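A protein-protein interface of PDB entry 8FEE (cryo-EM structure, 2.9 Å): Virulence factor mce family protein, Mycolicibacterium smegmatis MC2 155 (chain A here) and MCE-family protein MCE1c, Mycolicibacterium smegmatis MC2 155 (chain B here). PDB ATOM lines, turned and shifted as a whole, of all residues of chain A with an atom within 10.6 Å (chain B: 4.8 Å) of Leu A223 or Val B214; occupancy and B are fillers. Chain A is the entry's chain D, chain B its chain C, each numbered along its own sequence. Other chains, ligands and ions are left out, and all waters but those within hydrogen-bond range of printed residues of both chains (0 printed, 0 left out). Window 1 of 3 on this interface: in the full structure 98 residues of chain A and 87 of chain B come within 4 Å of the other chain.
Of the printed residues of chain B, Leu A218 touches Ser B211 (3.5 Å). Of the printed residues of chain B, Phe A219 touches Ser B211 (3.1 Å). Of the printed residues of chain B, Ala A222 touches Ser B211 and Asn B215. Of chain B, only Ser B211, Val B214 and Asn B215 come within 4 Å of Leu A223. Of the printed residues of chain B, Ser A226 touches Asn B215. Of chain A, only Leu A223 (3.8 Å) comes within 4 Å of Val B214. Leu B217 touches none of the printed residues of chain A.
Of the 9 printed residues of chain B, 4 touch a printed residue of chain A. Hydrophobic or aromatic side chains of chain B within 4 Å of the printed part of chain A: Val B214 and Leu B218. Along chain A the printed residues that touch a printed residue of chain B span positions 218 to 233. Among the printed residues, 10 pairs touch across the chains. Among the printed residues, no Asp or Glu carboxylate lies within 4 Å of a Lys or Arg side-chain nitrogen of the other chain.
OG of Ser B211 lies close to O of Phe A219. OD1 of Asn B215 lies within hydrogen-bond range of OG of Ser A226 (3.3 Å).
O of Leu A218 touches OG of Ser B211 (3.5 Å). CB of Ala A222 touches OG of Ser B211 (3.2 Å). Asn B215 touches Ala A222 (CG to O, 3.5 Å). Leu A223 touches Ser B211 (CD1 to OG, 3.3 Å). CD2 of Leu A223 touches CG1 of Val B214 (3.8 Å). Leu A223 touches Asn B215 (CD1 to CB, 3.9 Å). CD1 of Leu B218 touches CE1 of Phe A230 (3.7 Å). CD2 of Leu A233 touches O of Leu B218, at 3.5 Å.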
ATOM      1  N   SER A 215     -23.456  10.692 -31.393  1.00  0.00           N
ATOM      2  CA  SER A 215     -23.044  10.469 -30.010  1.00  0.00           C
ATOM      3  C   SER A 215     -21.530  10.320 -29.888  1.00  0.00           C
ATOM      4  O   SER A 215     -20.907  10.904 -28.989  1.00  0.00           O
ATOM      5  CB  SER A 215     -23.751   9.235 -29.451  1.00  0.00           C
ATOM      6  OG  SER A 215     -25.157   9.381 -29.524  1.00  0.00           O
ATOM      7  N   LEU A 216     -20.924   9.531 -30.780  1.00  0.00           N
ATOM      8  CA  LEU A 216     -19.473   9.421 -30.812  1.00  0.00           C
ATOM      9  C   LEU A 216     -18.815  10.762 -31.091  1.00  0.00           C
ATOM     10  O   LEU A 216     -17.697  11.003 -30.630  1.00  0.00           O
ATOM     11  CB  LEU A 216     -19.041   8.396 -31.861  1.00  0.00           C
ATOM     12  CG  LEU A 216     -19.327   6.926 -31.552  1.00  0.00           C
ATOM     13  CD1 LEU A 216     -18.870   6.041 -32.699  1.00  0.00           C
ATOM     14  CD2 LEU A 216     -18.656   6.513 -30.255  1.00  0.00           C
ATOM     15  N   ALA A 217     -19.486  11.648 -31.832  1.00  0.00           N
ATOM     16  CA  ALA A 217     -18.934  12.978 -32.062  1.00  0.00           C
ATOM     17  C   ALA A 217     -18.753  13.730 -30.752  1.00  0.00           C
ATOM     18  O   ALA A 217     -17.688  14.297 -30.497  1.00  0.00           O
ATOM     19  CB  ALA A 217     -19.836  13.761 -33.013  1.00  0.00           C
ATOM     20  N   LEU A 218     -19.780  13.729 -29.897  1.00  0.00           N
ATOM     21  CA  LEU A 218     -19.655  14.389 -28.601  1.00  0.00           C
ATOM     22  C   LEU A 218     -18.621  13.693 -27.726  1.00  0.00           C
ATOM     23  O   LEU A 218     -17.817  14.358 -27.056  1.00  0.00           O
ATOM     24  CB  LEU A 218     -21.010  14.436 -27.893  1.00  0.00           C
ATOM     25  CG  LEU A 218     -21.907  15.648 -28.158  1.00  0.00           C
ATOM     26  CD1 LEU A 218     -22.527  15.597 -29.544  1.00  0.00           C
ATOM     27  CD2 LEU A 218     -22.984  15.756 -27.089  1.00  0.00           C
ATOM     28  N   PHE A 219     -18.625  12.356 -27.727  1.00  0.00           N
ATOM     29  CA  PHE A 219     -17.658  11.604 -26.930  1.00  0.00           C
ATOM     30  C   PHE A 219     -16.227  11.983 -27.295  1.00  0.00           C
ATOM     31  O   PHE A 219     -15.409  12.313 -26.425  1.00  0.00           O
ATOM     32  CB  PHE A 219     -17.888  10.104 -27.118  1.00  0.00           C
ATOM     33  CG  PHE A 219     -16.885   9.241 -26.410  1.00  0.00           C
ATOM     34  CD1 PHE A 219     -16.909   9.114 -25.033  1.00  0.00           C
ATOM     35  CD2 PHE A 219     -15.926   8.545 -27.124  1.00  0.00           C
ATOM     36  CE1 PHE A 219     -15.990   8.317 -24.381  1.00  0.00           C
ATOM     37  CE2 PHE A 219     -15.003   7.747 -26.478  1.00  0.00           C
ATOM     38  CZ  PHE A 219     -15.036   7.632 -25.105  1.00  0.00           C
ATOM     39  N   VAL A 220     -15.922  11.978 -28.592  1.00  0.00           N
ATOM     40  CA  VAL A 220     -14.568  12.261 -29.047  1.00  0.00           C
ATOM     41  C   VAL A 220     -14.225  13.733 -28.851  1.00  0.00           C
ATOM     42  O   VAL A 220     -13.116  14.067 -28.420  1.00  0.00           O
ATOM     43  CB  VAL A 220     -14.410  11.818 -30.511  1.00  0.00           C
ATOM     44  CG1 VAL A 220     -13.056  12.160 -30.999  1.00  0.00           C
ATOM     45  CG2 VAL A 220     -14.613  10.320 -30.626  1.00  0.00           C
ATOM     46  N   ASN A 221     -15.166  14.640 -29.141  1.00  0.00           N
ATOM     47  CA  ASN A 221     -14.911  16.063 -28.947  1.00  0.00           C
ATOM     48  C   ASN A 221     -14.677  16.412 -27.487  1.00  0.00           C
ATOM     49  O   ASN A 221     -14.047  17.436 -27.202  1.00  0.00           O
ATOM     50  CB  ASN A 221     -16.068  16.900 -29.493  1.00  0.00           C
ATOM     51  CG  ASN A 221     -16.162  16.850 -31.001  1.00  0.00           C
ATOM     52  OD1 ASN A 221     -15.198  16.503 -31.681  1.00  0.00           O
ATOM     53  ND2 ASN A 221     -17.328  17.198 -31.533  1.00  0.00           N
ATOM     54  N   ALA A 222     -15.184  15.608 -26.557  1.00  0.00           N
ATOM     55  CA  ALA A 222     -14.907  15.873 -25.154  1.00  0.00           C
ATOM     56  C   ALA A 222     -13.671  15.148 -24.641  1.00  0.00           C
ATOM     57  O   ALA A 222     -13.068  15.605 -23.664  1.00  0.00           O
ATOM     58  CB  ALA A 222     -16.115  15.498 -24.293  1.00  0.00           C
ATOM     59  N   LEU A 223     -13.274  14.037 -25.266  1.00  0.00           N
ATOM     60  CA  LEU A 223     -12.125  13.269 -24.796  1.00  0.00           C
ATOM     61  C   LEU A 223     -10.871  13.417 -25.656  1.00  0.00           C
ATOM     62  O   LEU A 223      -9.921  12.654 -25.463  1.00  0.00           O
ATOM     63  CB  LEU A 223     -12.484  11.786 -24.686  1.00  0.00           C
ATOM     64  CG  LEU A 223     -12.989  11.300 -23.329  1.00  0.00           C
ATOM     65  CD1 LEU A 223     -14.421  11.736 -23.097  1.00  0.00           C
ATOM     66  CD2 LEU A 223     -12.855   9.792 -23.223  1.00  0.00           C
ATOM     67  N   HIS A 224     -10.824  14.367 -26.589  1.00  0.00           N
ATOM     68  CA  HIS A 224      -9.669  14.416 -27.481  1.00  0.00           C
ATOM     69  C   HIS A 224      -8.529  15.278 -26.954  1.00  0.00           C
ATOM     70  O   HIS A 224      -7.363  14.985 -27.242  1.00  0.00           O
ATOM     71  CB  HIS A 224     -10.083  14.911 -28.873  1.00  0.00           C
ATOM     72  CG  HIS A 224     -10.301  16.389 -28.959  1.00  0.00           C
ATOM     73  ND1 HIS A 224      -9.365  17.249 -29.492  1.00  0.00           N
ATOM     74  CD2 HIS A 224     -11.347  17.161 -28.581  1.00  0.00           C
ATOM     75  CE1 HIS A 224      -9.827  18.486 -29.443  1.00  0.00           C
ATOM     76  NE2 HIS A 224     -11.027  18.460 -28.892  1.00  0.00           N
ATOM     77  N   ARG A 225      -8.830  16.330 -26.191  1.00  0.00           N
ATOM     78  CA  ARG A 225      -7.795  17.269 -25.769  1.00  0.00           C
ATOM     79  C   ARG A 225      -6.868  16.705 -24.699  1.00  0.00           C
ATOM     80  O   ARG A 225      -5.791  17.267 -24.478  1.00  0.00           O
ATOM     81  CB  ARG A 225      -8.434  18.557 -25.249  1.00  0.00           C
ATOM     82  CG  ARG A 225      -8.834  19.538 -26.332  1.00  0.00           C
ATOM     83  CD  ARG A 225      -9.137  20.906 -25.751  1.00  0.00           C
ATOM     84  NE  ARG A 225      -9.114  21.947 -26.772  1.00  0.00           N
ATOM     85  CZ  ARG A 225      -8.018  22.572 -27.181  1.00  0.00           C
ATOM     86  NH1 ARG A 225      -6.829  22.282 -26.680  1.00  0.00           N
ATOM     87  NH2 ARG A 225      -8.118  23.509 -28.119  1.00  0.00           N
ATOM     88  N   SER A 226      -7.252  15.618 -24.028  1.00  0.00           N
ATOM     89  CA  SER A 226      -6.486  15.090 -22.906  1.00  0.00           C
ATOM     90  C   SER A 226      -5.634  13.874 -23.263  1.00  0.00           C
ATOM     91  O   SER A 226      -5.481  12.975 -22.429  1.00  0.00           O
ATOM     92  CB  SER A 226      -7.433  14.750 -21.756  1.00  0.00           C
ATOM     93  OG  SER A 226      -8.212  15.876 -21.389  1.00  0.00           O
ATOM     94  N   ASP A 227      -5.092  13.810 -24.483  1.00  0.00           N
ATOM     95  CA  ASP A 227      -4.365  12.612 -24.904  1.00  0.00           C
ATOM     96  C   ASP A 227      -3.128  12.382 -24.041  1.00  0.00           C
ATOM     97  O   ASP A 227      -2.848  11.248 -23.616  1.00  0.00           O
ATOM     98  CB  ASP A 227      -3.981  12.722 -26.379  1.00  0.00           C
ATOM     99  CG  ASP A 227      -3.367  14.062 -26.721  1.00  0.00           C
ATOM    100  OD1 ASP A 227      -3.404  14.969 -25.863  1.00  0.00           O
ATOM    101  OD2 ASP A 227      -2.844  14.210 -27.845  1.00  0.00           O
ATOM    102  N   GLN A 228      -2.405  13.460 -23.719  1.00  0.00           N
ATOM    103  CA  GLN A 228      -1.258  13.309 -22.838  1.00  0.00           C
ATOM    104  C   GLN A 228      -1.714  12.978 -21.430  1.00  0.00           C
ATOM    105  O   GLN A 228      -1.005  12.277 -20.699  1.00  0.00           O
ATOM    106  CB  GLN A 228      -0.408  14.580 -22.848  1.00  0.00           C
ATOM    107  CG  GLN A 228      -0.028  15.075 -24.239  1.00  0.00           C
ATOM    108  CD  GLN A 228       0.676  14.022 -25.079  1.00  0.00           C
ATOM    109  OE1 GLN A 228       1.424  13.190 -24.564  1.00  0.00           O
ATOM    110  NE2 GLN A 228       0.436  14.055 -26.385  1.00  0.00           N
ATOM    111  N   GLN A 229      -2.886  13.479 -21.029  1.00  0.00           N
ATOM    112  CA  GLN A 229      -3.405  13.138 -19.712  1.00  0.00           C
ATOM    113  C   GLN A 229      -3.691  11.646 -19.641  1.00  0.00           C
ATOM    114  O   GLN A 229      -3.483  11.014 -18.603  1.00  0.00           O
ATOM    115  CB  GLN A 229      -4.659  13.952 -19.404  1.00  0.00           C
ATOM    116  CG  GLN A 229      -4.523  15.432 -19.711  1.00  0.00           C
ATOM    117  CD  GLN A 229      -3.633  16.150 -18.722  1.00  0.00           C
ATOM    118  OE1 GLN A 229      -3.434  15.689 -17.599  1.00  0.00           O
ATOM    119  NE2 GLN A 229      -3.091  17.290 -19.133  1.00  0.00           N
ATOM    120  N   PHE A 230      -4.169  11.066 -20.747  1.00  0.00           N
ATOM    121  CA  PHE A 230      -4.452   9.633 -20.783  1.00  0.00           C
ATOM    122  C   PHE A 230      -3.168   8.819 -20.723  1.00  0.00           C
ATOM    123  O   PHE A 230      -3.116   7.778 -20.056  1.00  0.00           O
ATOM    124  CB  PHE A 230      -5.257   9.261 -22.029  1.00  0.00           C
ATOM    125  CG  PHE A 230      -6.549  10.014 -22.180  1.00  0.00           C
ATOM    126  CD1 PHE A 230      -7.168  10.607 -21.090  1.00  0.00           C
ATOM    127  CD2 PHE A 230      -7.153  10.117 -23.418  1.00  0.00           C
ATOM    128  CE1 PHE A 230      -8.352  11.293 -21.238  1.00  0.00           C
ATOM    129  CE2 PHE A 230      -8.336  10.798 -23.571  1.00  0.00           C
ATOM    130  CZ  PHE A 230      -8.938  11.388 -22.481  1.00  0.00           C
ATOM    131  N   VAL A 231      -2.121   9.274 -21.421  1.00  0.00           N
ATOM    132  CA  VAL A 231      -0.836   8.578 -21.337  1.00  0.00           C
ATOM    133  C   VAL A 231      -0.281   8.652 -19.918  1.00  0.00           C
ATOM    134  O   VAL A 231       0.216   7.656 -19.371  1.00  0.00           O
ATOM    135  CB  VAL A 231       0.151   9.162 -22.365  1.00  0.00           C
ATOM    136  CG1 VAL A 231       1.524   8.534 -22.210  1.00  0.00           C
ATOM    137  CG2 VAL A 231      -0.373   8.955 -23.774  1.00  0.00           C
ATOM    138  N   LEU A 233      -2.080   8.975 -17.235  1.00  0.00           N
ATOM    139  CA  LEU A 233      -2.940   8.133 -16.411  1.00  0.00           C
ATOM    140  C   LEU A 233      -2.548   6.669 -16.519  1.00  0.00           C
ATOM    141  O   LEU A 233      -2.489   5.964 -15.509  1.00  0.00           O
ATOM    142  CB  LEU A 233      -4.400   8.322 -16.824  1.00  0.00           C
ATOM    143  CG  LEU A 233      -5.440   7.347 -16.267  1.00  0.00           C
ATOM    144  CD1 LEU A 233      -5.462   7.352 -14.748  1.00  0.00           C
ATOM    145  CD2 LEU A 233      -6.813   7.677 -16.824  1.00  0.00           C
ATOM    146  N   ARG B 210     -22.679  10.989 -21.156  1.00  0.00           N
ATOM    147  CA  ARG B 210     -21.812  11.079 -19.989  1.00  0.00           C
ATOM    148  C   ARG B 210     -20.361  11.372 -20.357  1.00  0.00           C
ATOM    149  O   ARG B 210     -19.462  11.111 -19.551  1.00  0.00           O
ATOM    150  CB  ARG B 210     -21.901   9.790 -19.171  1.00  0.00           C
ATOM    151  CG  ARG B 210     -23.315   9.419 -18.767  1.00  0.00           C
ATOM    152  CD  ARG B 210     -23.982  10.560 -18.020  1.00  0.00           C
ATOM    153  NE  ARG B 210     -25.353  10.242 -17.642  1.00  0.00           N
ATOM    154  CZ  ARG B 210     -26.157  11.065 -16.984  1.00  0.00           C
ATOM    155  NH1 ARG B 210     -25.759  12.271 -16.614  1.00  0.00           N
ATOM    156  NH2 ARG B 210     -27.391  10.668 -16.689  1.00  0.00           N
ATOM    157  N   SER B 211     -20.117  11.910 -21.555  1.00  0.00           N
ATOM    158  CA  SER B 211     -18.751  12.063 -22.051  1.00  0.00           C
ATOM    159  C   SER B 211     -17.939  13.044 -21.213  1.00  0.00           C
ATOM    160  O   SER B 211     -16.755  12.804 -20.947  1.00  0.00           O
ATOM    161  CB  SER B 211     -18.768  12.508 -23.507  1.00  0.00           C
ATOM    162  OG  SER B 211     -17.444  12.623 -23.984  1.00  0.00           O
ATOM    163  N   THR B 212     -18.545  14.164 -20.813  1.00  0.00           N
ATOM    164  CA  THR B 212     -17.842  15.115 -19.956  1.00  0.00           C
ATOM    165  C   THR B 212     -17.471  14.472 -18.627  1.00  0.00           C
ATOM    166  O   THR B 212     -16.365  14.683 -18.107  1.00  0.00           O
ATOM    167  CB  THR B 212     -18.704  16.357 -19.735  1.00  0.00           C
ATOM    168  OG1 THR B 212     -19.012  16.956 -21.000  1.00  0.00           O
ATOM    169  CG2 THR B 212     -17.975  17.373 -18.871  1.00  0.00           C
ATOM    170  N   GLN B 213     -18.383  13.674 -18.068  1.00  0.00           N
ATOM    171  CA  GLN B 213     -18.076  12.934 -16.851  1.00  0.00           C
ATOM    172  C   GLN B 213     -16.926  11.960 -17.074  1.00  0.00           C
ATOM    173  O   GLN B 213     -16.064  11.811 -16.206  1.00  0.00           O
ATOM    174  CB  GLN B 213     -19.318  12.193 -16.354  1.00  0.00           C
ATOM    175  CG  GLN B 213     -20.291  13.063 -15.573  1.00  0.00           C
ATOM    176  CD  GLN B 213     -21.135  13.948 -16.465  1.00  0.00           C
ATOM    177  OE1 GLN B 213     -21.270  13.695 -17.662  1.00  0.00           O
ATOM    178  NE2 GLN B 213     -21.709  14.995 -15.887  1.00  0.00           N
ATOM    179  N   VAL B 214     -16.896  11.287 -18.229  1.00  0.00           N
ATOM    180  CA  VAL B 214     -15.807  10.355 -18.518  1.00  0.00           C
ATOM    181  C   VAL B 214     -14.472  11.090 -18.586  1.00  0.00           C
ATOM    182  O   VAL B 214     -13.461  10.629 -18.038  1.00  0.00           O
ATOM    183  CB  VAL B 214     -16.094   9.581 -19.819  1.00  0.00           C
ATOM    184  CG1 VAL B 214     -14.898   8.731 -20.209  1.00  0.00           C
ATOM    185  CG2 VAL B 214     -17.320   8.707 -19.654  1.00  0.00           C
ATOM    186  N   ASN B 215     -14.449  12.245 -19.255  1.00  0.00           N
ATOM    187  CA  ASN B 215     -13.217  13.019 -19.372  1.00  0.00           C
ATOM    188  C   ASN B 215     -12.725  13.478 -18.005  1.00  0.00           C
ATOM    189  O   ASN B 215     -11.536  13.342 -17.678  1.00  0.00           O
ATOM    190  CB  ASN B 215     -13.441  14.218 -20.293  1.00  0.00           C
ATOM    191  CG  ASN B 215     -12.288  15.198 -20.262  1.00  0.00           C
ATOM    192  OD1 ASN B 215     -11.126  14.810 -20.380  1.00  0.00           O
ATOM    193  ND2 ASN B 215     -12.603  16.477 -20.095  1.00  0.00           N
ATOM    194  N   GLN B 216     -13.630  14.035 -17.195  1.00  0.00           N
ATOM    195  CA  GLN B 216     -13.238  14.507 -15.872  1.00  0.00           C
ATOM    196  C   GLN B 216     -12.798  13.347 -14.989  1.00  0.00           C
ATOM    197  O   GLN B 216     -11.837  13.474 -14.221  1.00  0.00           O
ATOM    198  CB  GLN B 216     -14.389  15.279 -15.230  1.00  0.00           C
ATOM    199  CG  GLN B 216     -13.941  16.342 -14.248  1.00  0.00           C
ATOM    200  CD  GLN B 216     -15.022  17.365 -13.972  1.00  0.00           C
ATOM    201  OE1 GLN B 216     -16.153  17.229 -14.437  1.00  0.00           O
ATOM    202  NE2 GLN B 216     -14.677  18.399 -13.215  1.00  0.00           N
ATOM    203  N   LEU B 217     -13.478  12.205 -15.105  1.00  0.00           N
ATOM    204  CA  LEU B 217     -13.084  10.995 -14.394  1.00  0.00           C
ATOM    205  C   LEU B 217     -11.652  10.611 -14.731  1.00  0.00           C
ATOM    206  O   LEU B 217     -10.839  10.366 -13.835  1.00  0.00           O
ATOM    207  CB  LEU B 217     -14.060   9.868 -14.747  1.00  0.00           C
ATOM    208  CG  LEU B 217     -14.014   8.431 -14.213  1.00  0.00           C
ATOM    209  CD1 LEU B 217     -15.363   7.795 -14.482  1.00  0.00           C
ATOM    210  CD2 LEU B 217     -12.927   7.573 -14.846  1.00  0.00           C
ATOM    211  N   LEU B 218     -11.327  10.553 -16.024  1.00  0.00           N
ATOM    212  CA  LEU B 218      -9.990  10.125 -16.427  1.00  0.00           C
ATOM    213  C   LEU B 218      -8.922  11.108 -15.959  1.00  0.00           C
ATOM    214  O   LEU B 218      -7.877  10.692 -15.437  1.00  0.00           O
ATOM    215  CB  LEU B 218      -9.933   9.944 -17.943  1.00  0.00           C
ATOM    216  CG  LEU B 218     -10.763   8.789 -18.507  1.00  0.00           C
ATOM    217  CD1 LEU B 218     -10.586   8.677 -20.010  1.00  0.00           C
ATOM    218  CD2 LEU B 218     -10.395   7.485 -17.826  1.00  0.00           C
